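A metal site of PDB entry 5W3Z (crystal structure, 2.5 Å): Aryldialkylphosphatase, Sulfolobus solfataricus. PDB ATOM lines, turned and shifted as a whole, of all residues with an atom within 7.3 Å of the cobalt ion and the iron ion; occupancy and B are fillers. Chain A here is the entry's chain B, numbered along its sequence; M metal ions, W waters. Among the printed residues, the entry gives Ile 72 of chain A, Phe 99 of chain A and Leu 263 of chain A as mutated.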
ATOM      1  N   HIS A  22       2.863   5.809 -15.333  1.00  0.00           N
ATOM      2  CA  HIS A  22       1.970   4.747 -14.880  1.00  0.00           C
ATOM      3  C   HIS A  22       2.700   3.367 -14.869  1.00  0.00           C
ATOM      4  O   HIS A  22       2.677   2.605 -15.873  1.00  0.00           O
ATOM      5  CB  HIS A  22       0.773   4.735 -15.822  1.00  0.00           C
ATOM      6  CG  HIS A  22      -0.388   3.918 -15.368  1.00  0.00           C
ATOM      7  ND1 HIS A  22      -1.665   4.404 -15.399  1.00  0.00           N
ATOM      8  CD2 HIS A  22      -0.460   2.667 -14.850  1.00  0.00           C
ATOM      9  CE1 HIS A  22      -2.502   3.450 -15.019  1.00  0.00           C
ATOM     10  NE2 HIS A  22      -1.800   2.399 -14.652  1.00  0.00           N
ATOM     11  N   GLU A  23       3.381   3.061 -13.764  1.00  0.00           N
ATOM     12  CA  GLU A  23       3.944   1.715 -13.583  1.00  0.00           C
ATOM     13  C   GLU A  23       3.461   1.196 -12.227  1.00  0.00           C
ATOM     14  O   GLU A  23       3.242   1.988 -11.308  1.00  0.00           O
ATOM     15  CB  GLU A  23       5.471   1.717 -13.688  1.00  0.00           C
ATOM     16  CG  GLU A  23       6.068   2.423 -14.903  1.00  0.00           C
ATOM     17  CD  GLU A  23       5.642   1.802 -16.215  1.00  0.00           C
ATOM     18  OE1 GLU A  23       5.619   2.443 -17.282  1.00  0.00           O
ATOM     19  OE2 GLU A  23       5.295   0.631 -16.226  1.00  0.00           O
ATOM     20  N   HIS A  24       3.168  -0.091 -12.150  1.00  0.00           N
ATOM     21  CA  HIS A  24       2.903  -0.819 -10.901  1.00  0.00           C
ATOM     22  C   HIS A  24       4.125  -1.690 -10.434  1.00  0.00           C
ATOM     23  O   HIS A  24       4.523  -2.615 -11.112  1.00  0.00           O
ATOM     24  CB  HIS A  24       1.750  -1.760 -11.185  1.00  0.00           C
ATOM     25  CG  HIS A  24       0.495  -1.075 -11.623  1.00  0.00           C
ATOM     26  ND1 HIS A  24      -0.408  -0.494 -10.744  1.00  0.00           N
ATOM     27  CD2 HIS A  24      -0.018  -0.878 -12.873  1.00  0.00           C
ATOM     28  CE1 HIS A  24      -1.425  -0.004 -11.423  1.00  0.00           C
ATOM     29  NE2 HIS A  24      -1.204  -0.182 -12.725  1.00  0.00           N
ATOM     30  N   VAL A  27       0.735  -5.792  -7.971  1.00  0.00           N
ATOM     31  CA  VAL A  27      -0.705  -5.717  -8.091  1.00  0.00           C
ATOM     32  C   VAL A  27      -1.292  -6.987  -7.497  1.00  0.00           C
ATOM     33  O   VAL A  27      -0.800  -8.038  -7.800  1.00  0.00           O
ATOM     34  CB  VAL A  27      -1.128  -5.602  -9.564  1.00  0.00           C
ATOM     35  CG1 VAL A  27      -2.622  -5.475  -9.741  1.00  0.00           C
ATOM     36  CG2 VAL A  27      -0.665  -4.279 -10.142  1.00  0.00           C
ATOM     37  N   PRO A  67       0.361   3.964  -9.696  1.00  0.00           N
ATOM     38  CA  PRO A  67      -1.078   4.132  -9.381  1.00  0.00           C
ATOM     39  C   PRO A  67      -1.807   2.936  -8.802  1.00  0.00           C
ATOM     40  O   PRO A  67      -3.008   2.827  -8.866  1.00  0.00           O
ATOM     41  CB  PRO A  67      -1.694   4.648 -10.678  1.00  0.00           C
ATOM     42  CG  PRO A  67      -0.743   4.209 -11.732  1.00  0.00           C
ATOM     43  CD  PRO A  67       0.607   3.805 -11.125  1.00  0.00           C
ATOM     44  N   THR A  68      -1.074   2.034  -8.214  1.00  0.00           N
ATOM     45  CA  THR A  68      -1.666   0.986  -7.412  1.00  0.00           C
ATOM     46  C   THR A  68      -2.372   1.612  -6.179  1.00  0.00           C
ATOM     47  O   THR A  68      -1.677   2.219  -5.287  1.00  0.00           O
ATOM     48  CB  THR A  68      -0.515   0.044  -6.904  1.00  0.00           C
ATOM     49  OG1 THR A  68       0.323  -0.330  -8.027  1.00  0.00           O
ATOM     50  CG2 THR A  68      -1.150  -1.154  -6.247  1.00  0.00           C
ATOM     51  N   ILE A  72      -6.324  -2.882  -5.797  1.00  0.00           N
ATOM     52  CA  ILE A  72      -5.256  -3.567  -6.531  1.00  0.00           C
ATOM     53  C   ILE A  72      -3.974  -3.657  -5.711  1.00  0.00           C
ATOM     54  O   ILE A  72      -2.940  -3.906  -6.258  1.00  0.00           O
ATOM     55  CB  ILE A  72      -5.021  -2.962  -7.910  1.00  0.00           C
ATOM     56  CG1 ILE A  72      -4.802  -1.426  -7.822  1.00  0.00           C
ATOM     57  CG2 ILE A  72      -6.213  -3.258  -8.793  1.00  0.00           C
ATOM     58  CD1 ILE A  72      -4.529  -0.757  -9.173  1.00  0.00           C
ATOM     59  N   TYR A  97     -10.003   1.844  -6.990  1.00  0.00           N
ATOM     60  CA  TYR A  97     -10.048   1.253  -8.296  1.00  0.00           C
ATOM     61  C   TYR A  97     -11.138   0.230  -8.187  1.00  0.00           C
ATOM     62  O   TYR A  97     -10.887  -0.779  -7.594  1.00  0.00           O
ATOM     63  CB  TYR A  97      -8.748   0.515  -8.519  1.00  0.00           C
ATOM     64  CG  TYR A  97      -8.503  -0.133  -9.878  1.00  0.00           C
ATOM     65  CD1 TYR A  97      -9.180  -1.264 -10.243  1.00  0.00           C
ATOM     66  CD2 TYR A  97      -7.533   0.379 -10.770  1.00  0.00           C
ATOM     67  CE1 TYR A  97      -8.932  -1.866 -11.470  1.00  0.00           C
ATOM     68  CE2 TYR A  97      -7.257  -0.211 -11.995  1.00  0.00           C
ATOM     69  CZ  TYR A  97      -7.969  -1.358 -12.341  1.00  0.00           C
ATOM     70  OH  TYR A  97      -7.779  -2.034 -13.532  1.00  0.00           O
ATOM     71  N   PHE A  99     -14.787  -1.108 -10.790  1.00  0.00           N
ATOM     72  CA  PHE A  99     -15.487  -0.999 -12.064  1.00  0.00           C
ATOM     73  C   PHE A  99     -17.000  -0.944 -11.926  1.00  0.00           C
ATOM     74  O   PHE A  99     -17.654  -0.429 -12.835  1.00  0.00           O
ATOM     75  CB  PHE A  99     -15.127  -2.158 -13.052  1.00  0.00           C
ATOM     76  CG  PHE A  99     -13.715  -2.162 -13.577  1.00  0.00           C
ATOM     77  CD1 PHE A  99     -12.941  -1.021 -13.617  1.00  0.00           C
ATOM     78  CD2 PHE A  99     -13.193  -3.346 -14.083  1.00  0.00           C
ATOM     79  CE1 PHE A  99     -11.637  -1.086 -14.083  1.00  0.00           C
ATOM     80  CE2 PHE A  99     -11.886  -3.425 -14.569  1.00  0.00           C
ATOM     81  CZ  PHE A  99     -11.114  -2.294 -14.573  1.00  0.00           C
ATOM     82  N   KCX A 137      -6.148   8.342  -7.981  1.00  0.00           N
ATOM     83  CA  KCX A 137      -6.461   7.366  -9.059  1.00  0.00           C
ATOM     84  CB  KCX A 137      -5.625   6.052  -8.845  1.00  0.00           C
ATOM     85  CG  KCX A 137      -5.229   5.436 -10.172  1.00  0.00           C
ATOM     86  CD  KCX A 137      -6.227   4.632 -10.907  1.00  0.00           C
ATOM     87  CE  KCX A 137      -5.699   4.133 -12.224  1.00  0.00           C
ATOM     88  NZ  KCX A 137      -4.950   2.897 -12.063  1.00  0.00           N
ATOM     89  C   KCX A 137      -7.929   6.946  -8.948  1.00  0.00           C
ATOM     90  O   KCX A 137      -8.396   6.671  -7.803  1.00  0.00           O
ATOM     91  CX  KCX A 137      -4.718   2.074 -13.108  1.00  0.00           C
ATOM     92  OQ1 KCX A 137      -5.049   2.268 -14.280  1.00  0.00           O
ATOM     93  OQ2 KCX A 137      -3.961   1.010 -12.921  1.00  0.00           O
ATOM     94  N   ILE A 138      -8.608   6.806 -10.099  1.00  0.00           N
ATOM     95  CA  ILE A 138     -10.001   6.361 -10.187  1.00  0.00           C
ATOM     96  C   ILE A 138     -10.111   5.534 -11.421  1.00  0.00           C
ATOM     97  O   ILE A 138      -9.243   5.573 -12.245  1.00  0.00           O
ATOM     98  CB  ILE A 138     -11.015   7.553 -10.323  1.00  0.00           C
ATOM     99  CG1 ILE A 138     -10.705   8.493 -11.488  1.00  0.00           C
ATOM    100  CG2 ILE A 138     -10.973   8.478  -9.114  1.00  0.00           C
ATOM    101  CD1 ILE A 138     -11.583   8.172 -12.659  1.00  0.00           C
ATOM    102  N   ALA A 139     -11.176   4.778 -11.602  1.00  0.00           N
ATOM    103  CA  ALA A 139     -11.276   3.927 -12.770  1.00  0.00           C
ATOM    104  C   ALA A 139     -12.721   3.711 -13.251  1.00  0.00           C
ATOM    105  O   ALA A 139     -13.713   3.842 -12.438  1.00  0.00           O
ATOM    106  CB  ALA A 139     -10.699   2.602 -12.419  1.00  0.00           C
ATOM    107  N   ASP A 141     -14.400   0.946 -16.698  1.00  0.00           N
ATOM    108  CA  ASP A 141     -14.086   0.088 -17.856  1.00  0.00           C
ATOM    109  C   ASP A 141     -15.379  -0.355 -18.554  1.00  0.00           C
ATOM    110  O   ASP A 141     -16.280   0.478 -18.704  1.00  0.00           O
ATOM    111  CB  ASP A 141     -13.243  -1.081 -17.400  1.00  0.00           C
ATOM    112  CG  ASP A 141     -12.451  -1.711 -18.520  1.00  0.00           C
ATOM    113  OD1 ASP A 141     -12.951  -1.851 -19.651  1.00  0.00           O
ATOM    114  OD2 ASP A 141     -11.298  -2.087 -18.234  1.00  0.00           O
ATOM    115  N   THR A 169      -6.570   8.587 -14.312  1.00  0.00           N
ATOM    116  CA  THR A 169      -7.614   7.626 -14.458  1.00  0.00           C
ATOM    117  C   THR A 169      -7.176   6.405 -15.203  1.00  0.00           C
ATOM    118  O   THR A 169      -6.098   6.329 -15.763  1.00  0.00           O
ATOM    119  CB  THR A 169      -8.869   8.193 -15.203  1.00  0.00           C
ATOM    120  OG1 THR A 169      -8.629   8.231 -16.628  1.00  0.00           O
ATOM    121  CG2 THR A 169      -9.293   9.586 -14.687  1.00  0.00           C
ATOM    122  N   HIS A 170      -8.056   5.445 -15.110  1.00  0.00           N
ATOM    123  CA  HIS A 170      -8.134   4.195 -15.856  1.00  0.00           C
ATOM    124  C   HIS A 170      -9.471   4.217 -16.605  1.00  0.00           C
ATOM    125  O   HIS A 170     -10.517   4.466 -15.967  1.00  0.00           O
ATOM    126  CB  HIS A 170      -8.246   3.048 -14.857  1.00  0.00           C
ATOM    127  CG  HIS A 170      -8.526   1.737 -15.509  1.00  0.00           C
ATOM    128  ND1 HIS A 170      -7.547   0.762 -15.658  1.00  0.00           N
ATOM    129  CD2 HIS A 170      -9.642   1.262 -16.107  1.00  0.00           C
ATOM    130  CE1 HIS A 170      -8.095  -0.284 -16.266  1.00  0.00           C
ATOM    131  NE2 HIS A 170      -9.359  -0.007 -16.562  1.00  0.00           N
ATOM    132  N   SER A 171      -9.454   3.950 -17.917  1.00  0.00           N
ATOM    133  CA  SER A 171     -10.667   3.951 -18.748  1.00  0.00           C
ATOM    134  C   SER A 171     -10.604   2.827 -19.704  1.00  0.00           C
ATOM    135  O   SER A 171      -9.599   2.151 -19.803  1.00  0.00           O
ATOM    136  CB  SER A 171     -10.904   5.290 -19.486  1.00  0.00           C
ATOM    137  OG  SER A 171      -9.942   5.591 -20.502  1.00  0.00           O
ATOM    138  N   GLY A 198      -6.564   7.724 -18.759  1.00  0.00           N
ATOM    139  CA  GLY A 198      -5.667   6.600 -18.984  1.00  0.00           C
ATOM    140  C   GLY A 198      -6.181   5.647 -20.057  1.00  0.00           C
ATOM    141  O   GLY A 198      -7.379   5.606 -20.352  1.00  0.00           O
ATOM    142  N   HIS A 199      -5.229   4.894 -20.611  1.00  0.00           N
ATOM    143  CA  HIS A 199      -5.493   3.739 -21.426  1.00  0.00           C
ATOM    144  C   HIS A 199      -6.106   3.997 -22.766  1.00  0.00           C
ATOM    145  O   HIS A 199      -6.740   3.109 -23.318  1.00  0.00           O
ATOM    146  CB  HIS A 199      -6.352   2.704 -20.667  1.00  0.00           C
ATOM    147  CG  HIS A 199      -5.754   2.304 -19.385  1.00  0.00           C
ATOM    148  ND1 HIS A 199      -4.398   2.215 -19.214  1.00  0.00           N
ATOM    149  CD2 HIS A 199      -6.313   2.035 -18.184  1.00  0.00           C
ATOM    150  CE1 HIS A 199      -4.146   1.895 -17.956  1.00  0.00           C
ATOM    151  NE2 HIS A 199      -5.296   1.784 -17.312  1.00  0.00           N
ATOM    152  N   ASP A 222      -0.381   4.248 -22.488  1.00  0.00           N
ATOM    153  CA  ASP A 222       0.237   3.902 -21.243  1.00  0.00           C
ATOM    154  C   ASP A 222       0.277   2.365 -21.013  1.00  0.00           C
ATOM    155  O   ASP A 222       0.403   1.915 -19.899  1.00  0.00           O
ATOM    156  CB  ASP A 222      -0.401   4.763 -20.110  1.00  0.00           C
ATOM    157  CG  ASP A 222      -1.919   4.535 -19.936  1.00  0.00           C
ATOM    158  OD1 ASP A 222      -2.466   3.595 -20.564  1.00  0.00           O
ATOM    159  OD2 ASP A 222      -2.546   5.310 -19.152  1.00  0.00           O
ATOM    160  N   ARG A 223       0.260   1.598 -22.101  1.00  0.00           N
ATOM    161  CA  ARG A 223       0.192   0.153 -21.991  1.00  0.00           C
ATOM    162  C   ARG A 223       1.055  -0.569 -23.065  1.00  0.00           C
ATOM    163  O   ARG A 223       0.702  -1.578 -23.689  1.00  0.00           O
ATOM    164  CB  ARG A 223      -1.271  -0.268 -22.036  1.00  0.00           C
ATOM    165  CG  ARG A 223      -1.907  -0.412 -20.677  1.00  0.00           C
ATOM    166  CD  ARG A 223      -3.390  -0.638 -20.848  1.00  0.00           C
ATOM    167  NE  ARG A 223      -3.925  -1.106 -19.577  1.00  0.00           N
ATOM    168  CZ  ARG A 223      -5.157  -1.559 -19.375  1.00  0.00           C
ATOM    169  NH1 ARG A 223      -6.048  -1.615 -20.377  1.00  0.00           N
ATOM    170  NH2 ARG A 223      -5.500  -1.943 -18.151  1.00  0.00           N
ATOM    171  N   HIS A 255       4.183   1.960 -19.459  1.00  0.00           N
ATOM    172  CA  HIS A 255       3.948   0.522 -19.717  1.00  0.00           C
ATOM    173  C   HIS A 255       2.695  -0.112 -19.081  1.00  0.00           C
ATOM    174  O   HIS A 255       2.089  -1.019 -19.666  1.00  0.00           O
ATOM    175  CB  HIS A 255       5.174  -0.289 -19.338  1.00  0.00           C
ATOM    176  CG  HIS A 255       6.433   0.147 -19.991  1.00  0.00           C
ATOM    177  ND1 HIS A 255       7.271   1.060 -19.396  1.00  0.00           N
ATOM    178  CD2 HIS A 255       7.010  -0.198 -21.171  1.00  0.00           C
ATOM    179  CE1 HIS A 255       8.335   1.240 -20.170  1.00  0.00           C
ATOM    180  NE2 HIS A 255       8.195   0.485 -21.254  1.00  0.00           N
ATOM    181  N   ASP A 256       2.349   0.358 -17.890  1.00  0.00           N
ATOM    182  CA  ASP A 256       1.402  -0.297 -17.009  1.00  0.00           C
ATOM    183  C   ASP A 256       2.051  -1.540 -16.401  1.00  0.00           C
ATOM    184  O   ASP A 256       1.363  -2.457 -16.034  1.00  0.00           O
ATOM    185  CB  ASP A 256       0.039  -0.641 -17.704  1.00  0.00           C
ATOM    186  CG  ASP A 256      -1.194  -0.519 -16.753  1.00  0.00           C
ATOM    187  OD1 ASP A 256      -1.134  -0.125 -15.514  1.00  0.00           O
ATOM    188  OD2 ASP A 256      -2.280  -0.881 -17.299  1.00  0.00           O
ATOM    189  N   TYR A 257       3.390  -1.531 -16.400  1.00  0.00           N
ATOM    190  CA  TYR A 257       4.428  -2.332 -15.666  1.00  0.00           C
ATOM    191  C   TYR A 257       5.159  -3.425 -16.403  1.00  0.00           C
ATOM    192  O   TYR A 257       6.229  -3.874 -15.885  1.00  0.00           O
ATOM    193  CB  TYR A 257       4.134  -2.809 -14.242  1.00  0.00           C
ATOM    194  CG  TYR A 257       3.224  -3.997 -13.925  1.00  0.00           C
ATOM    195  CD1 TYR A 257       2.154  -4.378 -14.745  1.00  0.00           C
ATOM    196  CD2 TYR A 257       3.287  -4.604 -12.644  1.00  0.00           C
ATOM    197  CE1 TYR A 257       1.232  -5.322 -14.330  1.00  0.00           C
ATOM    198  CE2 TYR A 257       2.378  -5.563 -12.227  1.00  0.00           C
ATOM    199  CZ  TYR A 257       1.371  -5.919 -13.079  1.00  0.00           C
ATOM    200  OH  TYR A 257       0.540  -6.890 -12.662  1.00  0.00           O
ATOM    201  N   LEU A 263      -1.784  -7.137 -15.452  1.00  0.00           N
ATOM    202  CA  LEU A 263      -3.256  -6.965 -15.424  1.00  0.00           C
ATOM    203  C   LEU A 263      -3.873  -7.682 -16.681  1.00  0.00           C
ATOM    204  O   LEU A 263      -3.287  -8.639 -17.223  1.00  0.00           O
ATOM    205  CB  LEU A 263      -3.634  -5.423 -15.239  1.00  0.00           C
ATOM    206  CG  LEU A 263      -4.150  -4.831 -13.898  1.00  0.00           C
ATOM    207  CD1 LEU A 263      -4.065  -3.317 -13.791  1.00  0.00           C
ATOM    208  CD2 LEU A 263      -5.597  -5.280 -13.628  1.00  0.00           C
HETATM  209 CO    CO M   1      -5.387   0.793 -15.517  1.00  0.00          CO
HETATM  210 FE    FE M   2      -2.626   0.486 -14.169  1.00  0.00          FE
HETATM  211  O   HOH W   1      -3.978  -0.583 -15.483  1.00  0.00           O
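A ring nitrogen (ND1) of His 199 is in hydrogen-bond range of the guanidinium group of Arg 223 (3.4 Å). The side-chain carboxylate (OD1) of Asp 222 lies within hydrogen-bond range of a ring nitrogen (ND1) of His 199 (2.7 Å). The side-chain carboxylate (OD2) of Asp 256 lies within salt-bridge range of the guanidinium group (NE) of Arg 223 (2.8 Å). The backbone NH of Asp 256 sits at hydrogen-bond distance from the side-chain carboxylate of Glu 23 (3.4 Å). The backbone NH (N) of Asp 256 is in hydrogen-bond range of the backbone carbonyl oxygen (O) of Asp 222, at 3.2 Å. ND1 of His 24 sits at hydrogen-bond distance from OG1 of Thr 68 (2.8 Å). The backbone carbonyl oxygen (O) of Ile 138 lies within hydrogen-bond range of the backbone NH (N) of His 170. NE2 of His 170 lies within hydrogen-bond range of OD2 of Asp 141, 3.3 Å away.
Merely in contact with the cobalt ion: Arg 223. Six residues have an atom within 4 Å of the cobalt ion: His 22, KCX 137, His 170, His 199, Arg 223 and Asp 256.
Four residues have an atom within 4 Å of the iron ion: His 22, His 24, KCX 137 and Asp 256.
The cobalt ion is bound by OQ1 of KCX 137, water W1, NE2 of His 199 and ND1 of His 170.
The iron ion is bound by OQ2 of KCX 137 (1.9 Å), the side-chain carboxylate (OD1) of Asp 256 (2.1 Å), a ring nitrogen (NE2) of His 24 (2.1 Å), a ring nitrogen (NE2) of His 22 (2.1 Å) and water W1 (2.2 Å). The iron ion has five donor atoms within binding distance.
Water W1 lies within hydrogen-bond range of OD2 of Asp 256 and NH2 of Arg 223.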
